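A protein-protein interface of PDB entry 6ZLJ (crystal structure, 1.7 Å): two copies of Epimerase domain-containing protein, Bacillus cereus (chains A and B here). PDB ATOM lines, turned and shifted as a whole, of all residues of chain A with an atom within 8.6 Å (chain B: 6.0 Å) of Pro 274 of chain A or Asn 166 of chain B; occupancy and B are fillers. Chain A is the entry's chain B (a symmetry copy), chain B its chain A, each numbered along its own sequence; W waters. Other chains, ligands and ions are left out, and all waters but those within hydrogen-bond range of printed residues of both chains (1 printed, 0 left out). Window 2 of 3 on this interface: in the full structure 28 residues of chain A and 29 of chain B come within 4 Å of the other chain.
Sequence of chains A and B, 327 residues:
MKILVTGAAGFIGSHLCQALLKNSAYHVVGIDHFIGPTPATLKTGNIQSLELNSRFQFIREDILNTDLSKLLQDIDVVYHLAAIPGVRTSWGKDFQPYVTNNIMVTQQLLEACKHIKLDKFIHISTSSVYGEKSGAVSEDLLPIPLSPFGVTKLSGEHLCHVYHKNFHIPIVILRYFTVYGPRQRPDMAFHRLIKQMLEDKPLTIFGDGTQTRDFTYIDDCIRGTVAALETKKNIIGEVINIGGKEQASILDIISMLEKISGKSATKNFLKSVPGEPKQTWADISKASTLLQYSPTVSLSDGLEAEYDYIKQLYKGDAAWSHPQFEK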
ATOM      1  N   GLY A  86      15.388  32.728   3.671  1.00  0.00           N
ATOM      2  CA  GLY A  86      15.008  31.361   4.123  1.00  0.00           C
ATOM      3  C   GLY A  86      15.952  30.248   3.661  1.00  0.00           C
ATOM      4  O   GLY A  86      15.964  29.892   2.446  1.00  0.00           O
ATOM      5  N   VAL A  87      16.648  29.617   4.610  1.00  0.00           N
ATOM      6  CA  VAL A  87      17.616  28.512   4.344  1.00  0.00           C
ATOM      7  C   VAL A  87      16.874  27.358   3.661  1.00  0.00           C
ATOM      8  O   VAL A  87      17.493  26.714   2.835  1.00  0.00           O
ATOM      9  CB  VAL A  87      18.333  28.039   5.631  1.00  0.00           C
ATOM     10  CG1 VAL A  87      19.403  26.988   5.339  1.00  0.00           C
ATOM     11  CG2 VAL A  87      18.949  29.200   6.408  1.00  0.00           C
ATOM     12  N   ARG A  88      15.606  27.108   4.021  1.00  0.00           N
ATOM     13  CA  ARG A  88      14.859  25.844   3.742  1.00  0.00           C
ATOM     14  C   ARG A  88      13.990  25.914   2.468  1.00  0.00           C
ATOM     15  O   ARG A  88      13.595  24.837   1.966  1.00  0.00           O
ATOM     16  CB  ARG A  88      13.973  25.504   4.955  1.00  0.00           C
ATOM     17  CG  ARG A  88      14.709  25.474   6.294  1.00  0.00           C
ATOM     18  CD  ARG A  88      13.937  24.880   7.477  1.00  0.00           C
ATOM     19  NE  ARG A  88      13.244  25.880   8.282  1.00  0.00           N
ATOM     20  CZ  ARG A  88      13.817  26.696   9.166  1.00  0.00           C
ATOM     21  NH1 ARG A  88      13.073  27.566   9.831  1.00  0.00           N
ATOM     22  NH2 ARG A  88      15.117  26.640   9.389  1.00  0.00           N
ATOM     23  N   THR A  89      13.675  27.099   1.936  1.00  0.00           N
ATOM     24  CA  THR A  89      12.794  27.266   0.756  1.00  0.00           C
ATOM     25  C   THR A  89      13.599  27.751  -0.473  1.00  0.00           C
ATOM     26  O   THR A  89      13.062  28.534  -1.273  1.00  0.00           O
ATOM     27  CB  THR A  89      11.656  28.251   1.077  1.00  0.00           C
ATOM     28  OG1 THR A  89      12.278  29.410   1.622  1.00  0.00           O
ATOM     29  CG2 THR A  89      10.651  27.709   2.069  1.00  0.00           C
ATOM     30  N   SER A  90      14.845  27.297  -0.632  1.00  0.00           N
ATOM     31  CA  SER A  90      15.778  27.759  -1.698  1.00  0.00           C
ATOM     32  C   SER A  90      16.033  26.664  -2.740  1.00  0.00           C
ATOM     33  O   SER A  90      16.883  26.895  -3.595  1.00  0.00           O
ATOM     34  CB  SER A  90      17.071  28.273  -1.099  1.00  0.00           C
ATOM     35  OG  SER A  90      17.807  27.234  -0.465  1.00  0.00           O
ATOM     36  N   TRP A  91      15.274  25.562  -2.730  1.00  0.00           N
ATOM     37  CA  TRP A  91      15.434  24.421  -3.668  1.00  0.00           C
ATOM     38  C   TRP A  91      14.563  24.579  -4.928  1.00  0.00           C
ATOM     39  O   TRP A  91      13.527  25.302  -4.920  1.00  0.00           O
ATOM     40  CB  TRP A  91      15.124  23.104  -2.948  1.00  0.00           C
ATOM     41  CG  TRP A  91      15.945  22.905  -1.726  1.00  0.00           C
ATOM     42  CD1 TRP A  91      15.556  23.102  -0.434  1.00  0.00           C
ATOM     43  CD2 TRP A  91      17.309  22.455  -1.678  1.00  0.00           C
ATOM     44  NE1 TRP A  91      16.579  22.775   0.414  1.00  0.00           N
ATOM     45  CE2 TRP A  91      17.668  22.384  -0.314  1.00  0.00           C
ATOM     46  CE3 TRP A  91      18.257  22.101  -2.644  1.00  0.00           C
ATOM     47  CZ2 TRP A  91      18.943  22.000   0.105  1.00  0.00           C
ATOM     48  CZ3 TRP A  91      19.509  21.704  -2.226  1.00  0.00           C
ATOM     49  CH2 TRP A  91      19.850  21.657  -0.874  1.00  0.00           C
ATOM     50  N   ILE A 144      32.063  26.647   2.775  1.00  0.00           N
ATOM     51  CA  ILE A 144      31.419  25.683   1.848  1.00  0.00           C
ATOM     52  C   ILE A 144      29.954  25.565   2.233  1.00  0.00           C
ATOM     53  O   ILE A 144      29.571  24.742   3.068  1.00  0.00           O
ATOM     54  CB  ILE A 144      32.130  24.310   1.863  1.00  0.00           C
ATOM     55  CG1 ILE A 144      33.631  24.432   1.584  1.00  0.00           C
ATOM     56  CG2 ILE A 144      31.483  23.388   0.840  1.00  0.00           C
ATOM     57  CD1 ILE A 144      33.968  24.833   0.172  1.00  0.00           C
ATOM     58  N   PRO A 145      29.078  26.421   1.658  1.00  0.00           N
ATOM     59  CA  PRO A 145      27.676  26.423   2.060  1.00  0.00           C
ATOM     60  C   PRO A 145      27.022  25.053   1.855  1.00  0.00           C
ATOM     61  O   PRO A 145      27.426  24.331   0.983  1.00  0.00           O
ATOM     62  CB  PRO A 145      27.025  27.477   1.141  1.00  0.00           C
ATOM     63  CG  PRO A 145      28.168  28.360   0.698  1.00  0.00           C
ATOM     64  CD  PRO A 145      29.392  27.455   0.659  1.00  0.00           C
ATOM     65  N   LEU A 146      26.019  24.748   2.672  1.00  0.00           N
ATOM     66  CA  LEU A 146      25.208  23.505   2.610  1.00  0.00           C
ATOM     67  C   LEU A 146      23.898  23.730   1.850  1.00  0.00           C
ATOM     68  O   LEU A 146      23.202  22.754   1.558  1.00  0.00           O
ATOM     69  CB  LEU A 146      24.891  23.088   4.053  1.00  0.00           C
ATOM     70  CG  LEU A 146      25.990  22.335   4.802  1.00  0.00           C
ATOM     71  CD1 LEU A 146      25.485  21.942   6.180  1.00  0.00           C
ATOM     72  CD2 LEU A 146      26.442  21.090   4.040  1.00  0.00           C
ATOM     73  N   SER A 147      23.474  24.971   1.656  1.00  0.00           N
ATOM     74  CA  SER A 147      22.168  25.282   1.013  1.00  0.00           C
ATOM     75  C   SER A 147      22.337  26.226  -0.184  1.00  0.00           C
ATOM     76  O   SER A 147      23.259  27.040  -0.261  1.00  0.00           O
ATOM     77  CB  SER A 147      21.230  25.908   2.007  1.00  0.00           C
ATOM     78  OG  SER A 147      21.741  27.156   2.432  1.00  0.00           O
ATOM     79  N   PRO A 148      21.424  26.160  -1.172  1.00  0.00           N
ATOM     80  CA  PRO A 148      21.450  27.109  -2.280  1.00  0.00           C
ATOM     81  C   PRO A 148      21.374  28.551  -1.765  1.00  0.00           C
ATOM     82  O   PRO A 148      22.025  29.420  -2.338  1.00  0.00           O
ATOM     83  CB  PRO A 148      20.220  26.689  -3.092  1.00  0.00           C
ATOM     84  CG  PRO A 148      20.051  25.224  -2.755  1.00  0.00           C
ATOM     85  CD  PRO A 148      20.304  25.200  -1.276  1.00  0.00           C
ATOM     86  N   PHE A 206      12.596  19.804  13.686  1.00  0.00           N
ATOM     87  CA  PHE A 206      13.135  19.167  12.465  1.00  0.00           C
ATOM     88  C   PHE A 206      14.366  18.396  12.936  1.00  0.00           C
ATOM     89  O   PHE A 206      15.234  18.976  13.617  1.00  0.00           O
ATOM     90  CB  PHE A 206      13.391  20.194  11.358  1.00  0.00           C
ATOM     91  CG  PHE A 206      12.250  21.157  11.150  1.00  0.00           C
ATOM     92  CD1 PHE A 206      10.948  20.808  11.494  1.00  0.00           C
ATOM     93  CD2 PHE A 206      12.472  22.399  10.584  1.00  0.00           C
ATOM     94  CE1 PHE A 206       9.902  21.701  11.304  1.00  0.00           C
ATOM     95  CE2 PHE A 206      11.425  23.285  10.393  1.00  0.00           C
ATOM     96  CZ  PHE A 206      10.142  22.936  10.753  1.00  0.00           C
ATOM     97  N   LYS A 271      11.243  14.976  10.103  1.00  0.00           N
ATOM     98  CA  LYS A 271      12.520  14.689   9.381  1.00  0.00           C
ATOM     99  C   LYS A 271      13.367  15.969   9.308  1.00  0.00           C
ATOM    100  O   LYS A 271      12.794  17.060   9.107  1.00  0.00           O
ATOM    101  CB  LYS A 271      12.248  14.163   7.967  1.00  0.00           C
ATOM    102  CG  LYS A 271      11.549  12.813   7.908  1.00  0.00           C
ATOM    103  CD  LYS A 271      11.230  12.344   6.500  1.00  0.00           C
ATOM    104  CE  LYS A 271      10.562  10.982   6.478  1.00  0.00           C
ATOM    105  NZ  LYS A 271      10.316  10.515   5.092  1.00  0.00           N
ATOM    106  N   SER A 272      14.676  15.863   9.529  1.00  0.00           N
ATOM    107  CA  SER A 272      15.628  16.974   9.293  1.00  0.00           C
ATOM    108  C   SER A 272      15.429  17.479   7.852  1.00  0.00           C
ATOM    109  O   SER A 272      15.062  16.662   6.980  1.00  0.00           O
ATOM    110  CB  SER A 272      17.047  16.552   9.570  1.00  0.00           C
ATOM    111  OG  SER A 272      17.441  15.524   8.683  1.00  0.00           O
ATOM    112  N   VAL A 273      15.569  18.793   7.657  1.00  0.00           N
ATOM    113  CA  VAL A 273      15.471  19.523   6.355  1.00  0.00           C
ATOM    114  C   VAL A 273      16.848  19.522   5.703  1.00  0.00           C
ATOM    115  O   VAL A 273      17.838  19.852   6.364  1.00  0.00           O
ATOM    116  CB  VAL A 273      15.012  20.973   6.599  1.00  0.00           C
ATOM    117  CG1 VAL A 273      14.894  21.760   5.304  1.00  0.00           C
ATOM    118  CG2 VAL A 273      13.717  21.041   7.388  1.00  0.00           C
ATOM    119  N   PRO A 274      16.981  19.192   4.397  1.00  0.00           N
ATOM    120  CA  PRO A 274      18.275  19.322   3.731  1.00  0.00           C
ATOM    121  C   PRO A 274      18.760  20.776   3.741  1.00  0.00           C
ATOM    122  O   PRO A 274      17.958  21.710   3.642  1.00  0.00           O
ATOM    123  CB  PRO A 274      18.029  18.824   2.301  1.00  0.00           C
ATOM    124  CG  PRO A 274      16.535  18.908   2.110  1.00  0.00           C
ATOM    125  CD  PRO A 274      15.933  18.698   3.485  1.00  0.00           C
ATOM    126  N   GLY A 275      20.072  20.925   3.838  1.00  0.00           N
ATOM    127  CA  GLY A 275      20.782  22.196   3.657  1.00  0.00           C
ATOM    128  C   GLY A 275      21.000  22.952   4.952  1.00  0.00           C
ATOM    129  O   GLY A 275      21.424  24.095   4.840  1.00  0.00           O
ATOM    130  N   GLU A 276      20.757  22.349   6.120  1.00  0.00           N
ATOM    131  CA  GLU A 276      20.951  23.014   7.444  1.00  0.00           C
ATOM    132  C   GLU A 276      22.125  22.374   8.167  1.00  0.00           C
ATOM    133  O   GLU A 276      22.135  21.168   8.335  1.00  0.00           O
ATOM    134  CB  GLU A 276      19.714  22.839   8.314  1.00  0.00           C
ATOM    135  CG  GLU A 276      18.560  23.679   7.846  1.00  0.00           C
ATOM    136  CD  GLU A 276      17.471  23.827   8.877  1.00  0.00           C
ATOM    137  OE1 GLU A 276      17.230  22.839   9.589  1.00  0.00           O
ATOM    138  OE2 GLU A 276      16.826  24.901   8.917  1.00  0.00           O
ATOM    139  N   PRO A 277      23.093  23.150   8.700  1.00  0.00           N
ATOM    140  CA  PRO A 277      24.172  22.581   9.506  1.00  0.00           C
ATOM    141  C   PRO A 277      23.634  22.068  10.846  1.00  0.00           C
ATOM    142  O   PRO A 277      22.651  22.591  11.323  1.00  0.00           O
ATOM    143  CB  PRO A 277      25.093  23.780   9.771  1.00  0.00           C
ATOM    144  CG  PRO A 277      24.131  24.938   9.763  1.00  0.00           C
ATOM    145  CD  PRO A 277      23.154  24.620   8.647  1.00  0.00           C
ATOM    146  N   HIS B 161      28.871  21.303  -4.549  1.00  0.00           N
ATOM    147  CA  HIS B 161      29.052  20.810  -3.169  1.00  0.00           C
ATOM    148  C   HIS B 161      27.698  20.664  -2.481  1.00  0.00           C
ATOM    149  O   HIS B 161      27.497  19.703  -1.758  1.00  0.00           O
ATOM    150  CB  HIS B 161      30.035  21.701  -2.411  1.00  0.00           C
ATOM    151  CG  HIS B 161      31.427  21.583  -2.925  1.00  0.00           C
ATOM    152  ND1 HIS B 161      32.098  20.371  -2.944  1.00  0.00           N
ATOM    153  CD2 HIS B 161      32.283  22.497  -3.443  1.00  0.00           C
ATOM    154  CE1 HIS B 161      33.303  20.539  -3.466  1.00  0.00           C
ATOM    155  NE2 HIS B 161      33.458  21.838  -3.778  1.00  0.00           N
ATOM    156  N   VAL B 162      26.794  21.629  -2.643  1.00  0.00           N
ATOM    157  CA  VAL B 162      25.476  21.566  -1.966  1.00  0.00           C
ATOM    158  C   VAL B 162      24.746  20.293  -2.412  1.00  0.00           C
ATOM    159  O   VAL B 162      24.165  19.593  -1.522  1.00  0.00           O
ATOM    160  CB  VAL B 162      24.627  22.815  -2.272  1.00  0.00           C
ATOM    161  CG1 VAL B 162      23.174  22.597  -1.955  1.00  0.00           C
ATOM    162  CG2 VAL B 162      25.171  24.020  -1.558  1.00  0.00           C
ATOM    163  N   TYR B 163      24.732  19.996  -3.713  1.00  0.00           N
ATOM    164  CA  TYR B 163      23.927  18.878  -4.265  1.00  0.00           C
ATOM    165  C   TYR B 163      24.630  17.542  -3.975  1.00  0.00           C
ATOM    166  O   TYR B 163      23.915  16.536  -3.738  1.00  0.00           O
ATOM    167  CB  TYR B 163      23.551  19.158  -5.706  1.00  0.00           C
ATOM    168  CG  TYR B 163      22.403  20.130  -5.812  1.00  0.00           C
ATOM    169  CD1 TYR B 163      22.609  21.492  -5.699  1.00  0.00           C
ATOM    170  CD2 TYR B 163      21.112  19.700  -6.027  1.00  0.00           C
ATOM    171  CE1 TYR B 163      21.559  22.391  -5.808  1.00  0.00           C
ATOM    172  CE2 TYR B 163      20.056  20.588  -6.146  1.00  0.00           C
ATOM    173  CZ  TYR B 163      20.269  21.941  -6.018  1.00  0.00           C
ATOM    174  OH  TYR B 163      19.218  22.832  -6.118  1.00  0.00           O
ATOM    175  N   HIS B 164      25.949  17.551  -3.892  1.00  0.00           N
ATOM    176  CA  HIS B 164      26.739  16.381  -3.443  1.00  0.00           C
ATOM    177  C   HIS B 164      26.405  16.037  -1.982  1.00  0.00           C
ATOM    178  O   HIS B 164      25.993  14.914  -1.728  1.00  0.00           O
ATOM    179  CB  HIS B 164      28.222  16.616  -3.638  1.00  0.00           C
ATOM    180  CG  HIS B 164      29.073  15.514  -3.094  1.00  0.00           C
ATOM    181  ND1 HIS B 164      30.214  15.773  -2.378  1.00  0.00           N
ATOM    182  CD2 HIS B 164      28.983  14.172  -3.177  1.00  0.00           C
ATOM    183  CE1 HIS B 164      30.797  14.631  -2.034  1.00  0.00           C
ATOM    184  NE2 HIS B 164      30.072  13.642  -2.516  1.00  0.00           N
ATOM    185  N   LYS B 165      26.524  16.981  -1.062  1.00  0.00           N
ATOM    186  CA  LYS B 165      26.393  16.722   0.391  1.00  0.00           C
ATOM    187  C   LYS B 165      24.956  16.322   0.734  1.00  0.00           C
ATOM    188  O   LYS B 165      24.784  15.467   1.600  1.00  0.00           O
ATOM    189  CB  LYS B 165      26.863  17.936   1.187  1.00  0.00           C
ATOM    190  CG  LYS B 165      28.371  18.156   1.128  1.00  0.00           C
ATOM    191  CD  LYS B 165      28.912  19.003   2.258  1.00  0.00           C
ATOM    192  CE  LYS B 165      29.895  20.069   1.813  1.00  0.00           C
ATOM    193  NZ  LYS B 165      31.131  19.485   1.230  1.00  0.00           N
ATOM    194  N   ASN B 166      23.963  16.905   0.065  1.00  0.00           N
ATOM    195  CA  ASN B 166      22.536  16.756   0.404  1.00  0.00           C
ATOM    196  C   ASN B 166      21.933  15.583  -0.351  1.00  0.00           C
ATOM    197  O   ASN B 166      21.082  14.921   0.270  1.00  0.00           O
ATOM    198  CB  ASN B 166      21.744  18.042   0.172  1.00  0.00           C
ATOM    199  CG  ASN B 166      22.100  19.053   1.245  1.00  0.00           C
ATOM    200  OD1 ASN B 166      21.711  18.900   2.405  1.00  0.00           O
ATOM    201  ND2 ASN B 166      22.906  20.040   0.892  1.00  0.00           N
ATOM    202  N   PHE B 167      22.336  15.348  -1.606  1.00  0.00           N
ATOM    203  CA  PHE B 167      21.628  14.415  -2.524  1.00  0.00           C
ATOM    204  C   PHE B 167      22.557  13.388  -3.165  1.00  0.00           C
ATOM    205  O   PHE B 167      22.036  12.600  -3.989  1.00  0.00           O
ATOM    206  CB  PHE B 167      20.871  15.179  -3.596  1.00  0.00           C
ATOM    207  CG  PHE B 167      19.883  16.151  -3.018  1.00  0.00           C
ATOM    208  CD1 PHE B 167      18.824  15.704  -2.249  1.00  0.00           C
ATOM    209  CD2 PHE B 167      20.005  17.517  -3.249  1.00  0.00           C
ATOM    210  CE1 PHE B 167      17.913  16.605  -1.712  1.00  0.00           C
ATOM    211  CE2 PHE B 167      19.086  18.410  -2.716  1.00  0.00           C
ATOM    212  CZ  PHE B 167      18.051  17.957  -1.942  1.00  0.00           C
ATOM    213  N   HIS B 168      23.829  13.375  -2.788  1.00  0.00           N
ATOM    214  CA  HIS B 168      24.825  12.350  -3.183  1.00  0.00           C
ATOM    215  C   HIS B 168      25.079  12.416  -4.695  1.00  0.00           C
ATOM    216  O   HIS B 168      25.479  11.382  -5.272  1.00  0.00           O
ATOM    217  CB  HIS B 168      24.357  10.949  -2.754  1.00  0.00           C
ATOM    218  CG  HIS B 168      23.769  10.908  -1.382  1.00  0.00           C
ATOM    219  ND1 HIS B 168      24.530  11.151  -0.239  1.00  0.00           N
ATOM    220  CD2 HIS B 168      22.501  10.700  -0.964  1.00  0.00           C
ATOM    221  CE1 HIS B 168      23.754  11.062   0.826  1.00  0.00           C
ATOM    222  NE2 HIS B 168      22.494  10.800   0.406  1.00  0.00           N
HETATM  223  O   HOH W   1      18.218  25.269  -5.596  1.00  0.00           O
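The side-chain amide oxygen of Asn 166 of chain B lies within hydrogen-bond range of the backbone NH of Gly 275 of chain A, at 3.0 Å. The side-chain amide nitrogen (ND2) of Asn 166 of chain B is in hydrogen-bond range of the backbone carbonyl oxygen (O) of Leu 146 of chain A, 2.8 Å away.
The side-chain amide nitrogen (ND2) of Asn 166 of chain B is in hydrogen-bond range of the backbone carbonyl oxygen (O) of Val 162 of chain B (2.8 Å). The backbone carbonyl oxygen (O) of Tyr 163 of chain B lies within hydrogen-bond range of the backbone NH (N) of His 168 of chain B (3.3 Å).
Among the printed residues, pairs that only touch across the chains: Trp 91 of chain A with Val 162 of chain B (3.6 Å), Trp 91 of chain A with Tyr 163 of chain B (3.7 Å), Trp 91 of chain A with Asn 166 of chain B (3.9 Å), Trp 91 of chain A with Phe 167 of chain B (3.4 Å), Ile 144 of chain A with His 161 of chain B (3.9 Å), Ile 144 of chain A with Lys 165 of chain B (3.8 Å), Pro 145 of chain A with Val 162 of chain B (3.4 Å), Leu 146 of chain A with Val 162 of chain B (3.5 Å), Leu 146 of chain A with Lys 165 of chain B (3.7 Å), Ser 147 of chain A with Val 162 of chain B (3.8 Å), Pro 148 of chain A with Val 162 of chain B (3.9 Å) and Pro 274 of chain A with Asn 166 of chain B (3.7 Å).
Printed residues of chain B within 4 Å of Pro 145 of chain A: Val 162 (3.4 Å). Printed residues of chain B within 4 Å of Gly 275 of chain A: Asn 166. Printed residues of chain A within 4 Å of His 161 of chain B: Ile 144. Of the printed residues of chain A, Asn 166 of chain B touches Trp 91 (3.9 Å), Leu 146 (2.8 Å), Pro 274 (3.7 Å) and Gly 275 (3.0 Å). Of the printed residues of chain A, Phe 167 of chain B touches Trp 91 (3.4 Å). The nearest residue of chain B that does not touch Pro 274 of chain A is Phe 167 of chain B (4.3 Å). The nearest printed residue of chain B that does not touch Pro 145 of chain A is Lys 165 of chain B (5.0 Å).
Hydrophobic or aromatic side chains of chain A within 4 Å of the printed part of chain B: Trp 91, Ile 144, Leu 146, Pro 148 and Pro 274. Along chain A the printed residues that touch a printed residue of chain B span positions 91 to 275. Printed residues of chain B that touch a printed residue of chain A: His 161, Val 162, Tyr 163, Lys 165, Asn 166 and Phe 167. Among the printed residues, 14 pairs touch across the chains. Among the printed residues, no Asp or Glu carboxylate lies within 4 Å of a Lys or Arg side-chain nitrogen of the other chain.
No position is printed for both chains. Of the 14 pairs that touch across the chains among the printed residues, none has its exchanged pair printed and touching as well.
Water W1 bridges the side-chain hydroxyl of Tyr 163 of chain B and the backbone carbonyl oxygen of Ser 90 of chain A.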
